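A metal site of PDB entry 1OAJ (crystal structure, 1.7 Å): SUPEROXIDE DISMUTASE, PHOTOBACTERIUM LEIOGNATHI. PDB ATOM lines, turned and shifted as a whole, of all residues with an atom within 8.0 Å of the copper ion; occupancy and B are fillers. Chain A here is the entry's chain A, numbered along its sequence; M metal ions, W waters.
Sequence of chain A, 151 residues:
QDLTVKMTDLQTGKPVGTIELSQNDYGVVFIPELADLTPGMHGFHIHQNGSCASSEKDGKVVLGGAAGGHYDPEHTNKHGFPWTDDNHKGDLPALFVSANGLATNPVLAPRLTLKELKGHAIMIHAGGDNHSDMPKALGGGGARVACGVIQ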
ATOM      1  N   GLY A  43      -3.244  17.495  19.798  1.00  0.00           N
ATOM      2  CA  GLY A  43      -4.484  17.316  20.542  1.00  0.00           C
ATOM      3  C   GLY A  43      -5.345  18.517  20.192  1.00  0.00           C
ATOM      4  O   GLY A  43      -4.830  19.617  20.014  1.00  0.00           O
ATOM      5  N   PHE A  44      -6.653  18.313  20.102  1.00  0.00           N
ATOM      6  CA  PHE A  44      -7.616  19.336  19.720  1.00  0.00           C
ATOM      7  C   PHE A  44      -8.883  19.131  20.529  1.00  0.00           C
ATOM      8  O   PHE A  44      -9.647  18.218  20.253  1.00  0.00           O
ATOM      9  CB  PHE A  44      -7.898  19.184  18.237  1.00  0.00           C
ATOM     10  CG  PHE A  44      -8.618  20.304  17.561  1.00  0.00           C
ATOM     11  CD1 PHE A  44      -8.393  21.613  17.901  1.00  0.00           C
ATOM     12  CD2 PHE A  44      -9.563  20.019  16.582  1.00  0.00           C
ATOM     13  CE1 PHE A  44      -9.090  22.617  17.261  1.00  0.00           C
ATOM     14  CE2 PHE A  44     -10.238  21.017  15.943  1.00  0.00           C
ATOM     15  CZ  PHE A  44     -10.004  22.322  16.274  1.00  0.00           C
ATOM     16  N   HIS A  45      -9.140  19.962  21.541  1.00  0.00           N
ATOM     17  CA  HIS A  45     -10.370  19.771  22.339  1.00  0.00           C
ATOM     18  C   HIS A  45     -11.033  21.046  22.793  1.00  0.00           C
ATOM     19  O   HIS A  45     -10.449  22.119  22.816  1.00  0.00           O
ATOM     20  CB  HIS A  45     -10.072  18.985  23.595  1.00  0.00           C
ATOM     21  CG  HIS A  45      -8.778  18.163  23.564  1.00  0.00           C
ATOM     22  ND1 HIS A  45      -7.619  18.541  24.196  1.00  0.00           N
ATOM     23  CD2 HIS A  45      -8.513  16.984  22.961  1.00  0.00           C
ATOM     24  CE1 HIS A  45      -6.679  17.616  23.984  1.00  0.00           C
ATOM     25  NE2 HIS A  45      -7.201  16.662  23.229  1.00  0.00           N
ATOM     26  N   ILE A  46     -12.310  20.924  23.135  1.00  0.00           N
ATOM     27  CA  ILE A  46     -13.029  22.042  23.729  1.00  0.00           C
ATOM     28  C   ILE A  46     -12.709  21.976  25.192  1.00  0.00           C
ATOM     29  O   ILE A  46     -12.746  20.911  25.798  1.00  0.00           O
ATOM     30  CB  ILE A  46     -14.562  21.916  23.583  1.00  0.00           C
ATOM     31  CG1 ILE A  46     -14.957  21.706  22.110  1.00  0.00           C
ATOM     32  CG2 ILE A  46     -15.271  23.139  24.146  1.00  0.00           C
ATOM     33  CD1 ILE A  46     -14.013  22.368  21.121  1.00  0.00           C
ATOM     34  N   HIS A  47     -12.358  23.130  25.775  1.00  0.00           N
ATOM     35  CA  HIS A  47     -12.069  23.165  27.201  1.00  0.00           C
ATOM     36  C   HIS A  47     -13.208  23.872  27.921  1.00  0.00           C
ATOM     37  O   HIS A  47     -13.965  24.614  27.309  1.00  0.00           O
ATOM     38  CB  HIS A  47     -10.715  23.808  27.460  1.00  0.00           C
ATOM     39  CG  HIS A  47      -9.540  22.801  27.294  1.00  0.00           C
ATOM     40  ND1 HIS A  47      -8.727  22.463  28.346  1.00  0.00           N
ATOM     41  CD2 HIS A  47      -9.082  22.113  26.200  1.00  0.00           C
ATOM     42  CE1 HIS A  47      -7.813  21.602  27.919  1.00  0.00           C
ATOM     43  NE2 HIS A  47      -8.011  21.384  26.626  1.00  0.00           N
ATOM     44  N   GLY A  68      -9.387  25.815  31.933  1.00  0.00           N
ATOM     45  CA  GLY A  68      -9.874  24.655  32.646  1.00  0.00           C
ATOM     46  C   GLY A  68      -9.486  23.317  31.968  1.00  0.00           C
ATOM     47  O   GLY A  68      -8.558  23.246  31.158  1.00  0.00           O
ATOM     48  N   GLY A  69     -10.211  22.277  32.350  1.00  0.00           N
ATOM     49  CA  GLY A  69      -9.944  20.974  31.778  1.00  0.00           C
ATOM     50  C   GLY A  69     -10.862  20.763  30.595  1.00  0.00           C
ATOM     51  O   GLY A  69     -11.511  21.726  30.143  1.00  0.00           O
ATOM     52  N   HIS A  70     -10.944  19.545  30.091  1.00  0.00           N
ATOM     53  CA  HIS A  70     -11.810  19.295  28.941  1.00  0.00           C
ATOM     54  C   HIS A  70     -13.278  19.466  29.255  1.00  0.00           C
ATOM     55  O   HIS A  70     -13.729  19.148  30.368  1.00  0.00           O
ATOM     56  CB  HIS A  70     -11.589  17.903  28.381  1.00  0.00           C
ATOM     57  CG  HIS A  70     -10.190  17.704  27.758  1.00  0.00           C
ATOM     58  ND1 HIS A  70      -9.806  16.553  27.093  1.00  0.00           N
ATOM     59  CD2 HIS A  70      -9.120  18.531  27.710  1.00  0.00           C
ATOM     60  CE1 HIS A  70      -8.559  16.666  26.688  1.00  0.00           C
ATOM     61  NE2 HIS A  70      -8.120  17.861  27.048  1.00  0.00           N
ATOM     62  N   TYR A  71     -14.032  19.970  28.272  1.00  0.00           N
ATOM     63  CA  TYR A  71     -15.476  20.126  28.356  1.00  0.00           C
ATOM     64  C   TYR A  71     -16.012  18.747  28.653  1.00  0.00           C
ATOM     65  O   TYR A  71     -15.659  17.780  27.968  1.00  0.00           O
ATOM     66  CB  TYR A  71     -16.001  20.761  27.082  1.00  0.00           C
ATOM     67  CG  TYR A  71     -17.514  20.921  27.003  1.00  0.00           C
ATOM     68  CD1 TYR A  71     -18.231  21.543  28.018  1.00  0.00           C
ATOM     69  CD2 TYR A  71     -18.177  20.442  25.887  1.00  0.00           C
ATOM     70  CE1 TYR A  71     -19.611  21.647  27.892  1.00  0.00           C
ATOM     71  CE2 TYR A  71     -19.542  20.580  25.752  1.00  0.00           C
ATOM     72  CZ  TYR A  71     -20.237  21.183  26.764  1.00  0.00           C
ATOM     73  OH  TYR A  71     -21.591  21.333  26.644  1.00  0.00           O
ATOM     74  N   HIS A  79     -10.910  10.653  29.191  1.00  0.00           N
ATOM     75  CA  HIS A  79     -10.555  11.190  27.887  1.00  0.00           C
ATOM     76  C   HIS A  79     -10.728  10.067  26.868  1.00  0.00           C
ATOM     77  O   HIS A  79     -10.245   8.946  27.112  1.00  0.00           O
ATOM     78  CB  HIS A  79      -9.127  11.763  27.924  1.00  0.00           C
ATOM     79  CG  HIS A  79      -8.752  12.322  26.569  1.00  0.00           C
ATOM     80  ND1 HIS A  79      -9.203  13.535  26.109  1.00  0.00           N
ATOM     81  CD2 HIS A  79      -7.967  11.827  25.576  1.00  0.00           C
ATOM     82  CE1 HIS A  79      -8.748  13.763  24.886  1.00  0.00           C
ATOM     83  NE2 HIS A  79      -7.982  12.744  24.535  1.00  0.00           N
ATOM     84  N   HIS A  88     -15.100  12.887  27.819  1.00  0.00           N
ATOM     85  CA  HIS A  88     -15.359  14.283  27.561  1.00  0.00           C
ATOM     86  C   HIS A  88     -15.979  14.574  26.215  1.00  0.00           C
ATOM     87  O   HIS A  88     -15.414  14.203  25.184  1.00  0.00           O
ATOM     88  CB  HIS A  88     -14.060  15.083  27.570  1.00  0.00           C
ATOM     89  CG  HIS A  88     -13.070  14.738  28.696  1.00  0.00           C
ATOM     90  ND1 HIS A  88     -11.706  14.572  28.493  1.00  0.00           N
ATOM     91  CD2 HIS A  88     -13.284  14.597  30.023  1.00  0.00           C
ATOM     92  CE1 HIS A  88     -11.135  14.316  29.643  1.00  0.00           C
ATOM     93  NE2 HIS A  88     -12.073  14.338  30.591  1.00  0.00           N
ATOM     94  N   GLY A  90     -15.962  17.186  24.952  1.00  0.00           N
ATOM     95  CA  GLY A  90     -15.057  18.132  24.343  1.00  0.00           C
ATOM     96  C   GLY A  90     -14.031  17.482  23.430  1.00  0.00           C
ATOM     97  O   GLY A  90     -13.409  18.175  22.623  1.00  0.00           O
ATOM     98  N   ASP A  91     -13.842  16.151  23.510  1.00  0.00           N
ATOM     99  CA  ASP A  91     -12.818  15.437  22.709  1.00  0.00           C
ATOM    100  C   ASP A  91     -13.047  15.445  21.192  1.00  0.00           C
ATOM    101  O   ASP A  91     -13.980  14.801  20.699  1.00  0.00           O
ATOM    102  CB  ASP A  91     -12.696  14.002  23.215  1.00  0.00           C
ATOM    103  CG  ASP A  91     -12.287  13.960  24.680  1.00  0.00           C
ATOM    104  OD1 ASP A  91     -11.683  14.945  25.160  1.00  0.00           O
ATOM    105  OD2 ASP A  91     -12.567  12.942  25.346  1.00  0.00           O
ATOM    106  N   LEU A  92     -12.210  16.180  20.483  1.00  0.00           N
ATOM    107  CA  LEU A  92     -12.342  16.300  19.030  1.00  0.00           C
ATOM    108  C   LEU A  92     -11.329  15.428  18.270  1.00  0.00           C
ATOM    109  O   LEU A  92     -10.358  14.960  18.870  1.00  0.00           O
ATOM    110  CB  LEU A  92     -12.165  17.758  18.616  1.00  0.00           C
ATOM    111  CG  LEU A  92     -12.860  18.821  19.480  1.00  0.00           C
ATOM    112  CD1 LEU A  92     -12.163  20.164  19.312  1.00  0.00           C
ATOM    113  CD2 LEU A  92     -14.336  18.910  19.135  1.00  0.00           C
ATOM    114  N   ALA A 121     -13.705  27.191  25.398  1.00  0.00           N
ATOM    115  CA  ALA A 121     -12.553  27.541  24.637  1.00  0.00           C
ATOM    116  C   ALA A 121     -12.058  26.383  23.778  1.00  0.00           C
ATOM    117  O   ALA A 121     -12.158  25.222  24.176  1.00  0.00           O
ATOM    118  CB  ALA A 121     -11.433  28.022  25.550  1.00  0.00           C
ATOM    119  N   ILE A 122     -11.504  26.709  22.615  1.00  0.00           N
ATOM    120  CA  ILE A 122     -10.900  25.684  21.734  1.00  0.00           C
ATOM    121  C   ILE A 122      -9.403  25.681  22.035  1.00  0.00           C
ATOM    122  O   ILE A 122      -8.763  26.736  22.065  1.00  0.00           O
ATOM    123  CB  ILE A 122     -11.066  26.005  20.251  1.00  0.00           C
ATOM    124  CG1 ILE A 122     -12.515  26.277  19.860  1.00  0.00           C
ATOM    125  CG2 ILE A 122     -10.495  24.867  19.433  1.00  0.00           C
ATOM    126  CD1 ILE A 122     -12.744  26.310  18.363  1.00  0.00           C
ATOM    127  N   MET A 123      -8.852  24.517  22.278  1.00  0.00           N
ATOM    128  CA  MET A 123      -7.458  24.365  22.634  1.00  0.00           C
ATOM    129  C   MET A 123      -6.720  23.480  21.630  1.00  0.00           C
ATOM    130  O   MET A 123      -7.251  22.458  21.180  1.00  0.00           O
ATOM    131  CB  MET A 123      -7.367  23.752  24.022  1.00  0.00           C
ATOM    132  CG  MET A 123      -6.022  23.944  24.685  1.00  0.00           C
ATOM    133  SD  MET A 123      -5.754  25.661  25.204  1.00  0.00           S
ATOM    134  CE  MET A 123      -6.837  25.743  26.623  1.00  0.00           C
ATOM    135  N   ILE A 124      -5.491  23.872  21.299  1.00  0.00           N
ATOM    136  CA  ILE A 124      -4.614  23.107  20.434  1.00  0.00           C
ATOM    137  C   ILE A 124      -3.386  22.817  21.258  1.00  0.00           C
ATOM    138  O   ILE A 124      -2.736  23.740  21.774  1.00  0.00           O
ATOM    139  CB  ILE A 124      -4.216  23.851  19.138  1.00  0.00           C
ATOM    140  CG1 ILE A 124      -5.449  24.032  18.254  1.00  0.00           C
ATOM    141  CG2 ILE A 124      -3.144  23.091  18.397  1.00  0.00           C
ATOM    142  CD1 ILE A 124      -5.719  25.464  17.843  1.00  0.00           C
ATOM    143  N   HIS A 125      -3.049  21.553  21.367  1.00  0.00           N
ATOM    144  CA  HIS A 125      -1.922  21.187  22.187  1.00  0.00           C
ATOM    145  C   HIS A 125      -0.629  21.103  21.404  1.00  0.00           C
ATOM    146  O   HIS A 125      -0.553  21.456  20.227  1.00  0.00           O
ATOM    147  CB  HIS A 125      -2.256  19.863  22.943  1.00  0.00           C
ATOM    148  CG  HIS A 125      -3.352  20.070  24.024  1.00  0.00           C
ATOM    149  ND1 HIS A 125      -3.053  20.209  25.360  1.00  0.00           N
ATOM    150  CD2 HIS A 125      -4.684  20.196  23.893  1.00  0.00           C
ATOM    151  CE1 HIS A 125      -4.180  20.413  26.017  1.00  0.00           C
ATOM    152  NE2 HIS A 125      -5.177  20.396  25.145  1.00  0.00           N
ATOM    153  N   ASP A 129      -2.868  13.104  20.151  1.00  0.00           N
ATOM    154  CA  ASP A 129      -4.009  12.634  20.928  1.00  0.00           C
ATOM    155  C   ASP A 129      -4.331  11.165  20.602  1.00  0.00           C
ATOM    156  O   ASP A 129      -4.950  10.886  19.558  1.00  0.00           O
ATOM    157  CB  ASP A 129      -5.222  13.506  20.637  1.00  0.00           C
ATOM    158  CG  ASP A 129      -6.363  13.266  21.612  1.00  0.00           C
ATOM    159  OD1 ASP A 129      -6.351  12.243  22.306  1.00  0.00           O
ATOM    160  OD2 ASP A 129      -7.275  14.112  21.682  1.00  0.00           O
ATOM    161  N   LEU A 138      -4.836  12.656  29.208  1.00  0.00           N
ATOM    162  CA  LEU A 138      -5.426  13.445  28.173  1.00  0.00           C
ATOM    163  C   LEU A 138      -4.887  13.250  26.773  1.00  0.00           C
ATOM    164  O   LEU A 138      -4.661  14.218  26.048  1.00  0.00           O
ATOM    165  CB  LEU A 138      -5.370  14.903  28.611  1.00  0.00           C
ATOM    166  CG  LEU A 138      -5.892  15.080  30.033  1.00  0.00           C
ATOM    167  CD1 LEU A 138      -5.397  16.385  30.628  1.00  0.00           C
ATOM    168  CD2 LEU A 138      -7.398  15.021  30.045  1.00  0.00           C
ATOM    169  N   GLY A 141      -1.514  15.048  24.900  1.00  0.00           N
ATOM    170  CA  GLY A 141      -1.463  16.359  24.280  1.00  0.00           C
ATOM    171  C   GLY A 141      -0.459  17.289  24.954  1.00  0.00           C
ATOM    172  O   GLY A 141       0.179  18.115  24.299  1.00  0.00           O
ATOM    173  N   GLY A 142      -0.308  17.142  26.257  1.00  0.00           N
ATOM    174  CA  GLY A 142       0.634  17.944  27.004  1.00  0.00           C
ATOM    175  C   GLY A 142       0.311  19.417  26.975  1.00  0.00           C
ATOM    176  O   GLY A 142      -0.867  19.809  27.020  1.00  0.00           O
ATOM    177  N   ALA A 143       1.337  20.230  26.903  1.00  0.00           N
ATOM    178  CA  ALA A 143       1.216  21.687  26.904  1.00  0.00           C
ATOM    179  C   ALA A 143       0.193  22.226  25.931  1.00  0.00           C
ATOM    180  O   ALA A 143      -0.107  21.603  24.901  1.00  0.00           O
ATOM    181  CB  ALA A 143       2.573  22.309  26.619  1.00  0.00           C
ATOM    182  N   ARG A 144      -0.365  23.374  26.291  1.00  0.00           N
ATOM    183  CA  ARG A 144      -1.340  24.071  25.440  1.00  0.00           C
ATOM    184  C   ARG A 144      -0.550  25.052  24.604  1.00  0.00           C
ATOM    185  O   ARG A 144       0.216  25.842  25.148  1.00  0.00           O
ATOM    186  CB  ARG A 144      -2.401  24.820  26.294  1.00  0.00           C
ATOM    187  CG  ARG A 144      -3.367  23.885  27.043  1.00  0.00           C
ATOM    188  CD  ARG A 144      -3.879  24.451  28.373  1.00  0.00           C
ATOM    189  NE  ARG A 144      -4.314  23.384  29.295  1.00  0.00           N
ATOM    190  CZ  ARG A 144      -5.449  23.380  30.026  1.00  0.00           C
ATOM    191  NH1 ARG A 144      -6.290  24.396  29.935  1.00  0.00           N
ATOM    192  NH2 ARG A 144      -5.716  22.352  30.827  1.00  0.00           N
ATOM    193  N   ALA A 146      -2.077  26.793  21.475  1.00  0.00           N
ATOM    194  CA  ALA A 146      -2.920  27.770  20.792  1.00  0.00           C
ATOM    195  C   ALA A 146      -4.302  27.683  21.393  1.00  0.00           C
ATOM    196  O   ALA A 146      -4.744  26.594  21.772  1.00  0.00           O
ATOM    197  CB  ALA A 146      -2.972  27.494  19.287  1.00  0.00           C
HETATM  198 CU    CU M   1      -7.185  20.044  25.511  1.00  0.00          CU
HETATM  199 ZN    ZN M   2     -10.690  14.834  26.802  1.00  0.00          ZN
HETATM  200  O   HOH W   1      -5.833  19.141  28.337  1.00  0.00           O
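The guanidinium group (NH1) of Arg 144 sits at hydrogen-bond distance from a ring nitrogen (ND1) of His 47, at 3.5 Å.
A ring nitrogen (ND1) of His 47 sits close to the backbone carbonyl oxygen of Gly 69 (3.4 Å).
ND1 of His 47 sits at hydrogen-bond distance from O of Gly 68 (2.9 Å).
A ring nitrogen (ND1) of His 45 sits close to a ring nitrogen (NE2) of His 70.
N of Met 123 sits at hydrogen-bond distance from O of His 45 (2.9 Å).
OD2 of Asp 129 lies within hydrogen-bond range of NE2 of His 45 (3.0 Å).
N of His 125 is in hydrogen-bond range of O of Gly 43 (3.0 Å).
ND1 of His 125 lies within hydrogen-bond range of O of Gly 142, 2.8 Å away.
Met 123 touches the copper ion (CB to CU, 3.9999 Å).
Five residues have an atom within 4 Å of the copper ion: His 45, His 47, His 70, Met 123 and His 125.
Along chain A the residues within 4 Å of the copper ion span positions 45 to 125.
The nearest printed residue that does not touch the copper ion is Phe 44 (5.3 Å).
The copper ion is bound by NE2 of His 47 (1.9 Å), ND1 of His 45 (2.0 Å) and NE2 of His 125 (2.1 Å).
The copper ion has three donor atoms within binding distance.
Slightly farther from the copper ion lies NE2 of His 70 (2.8 Å).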
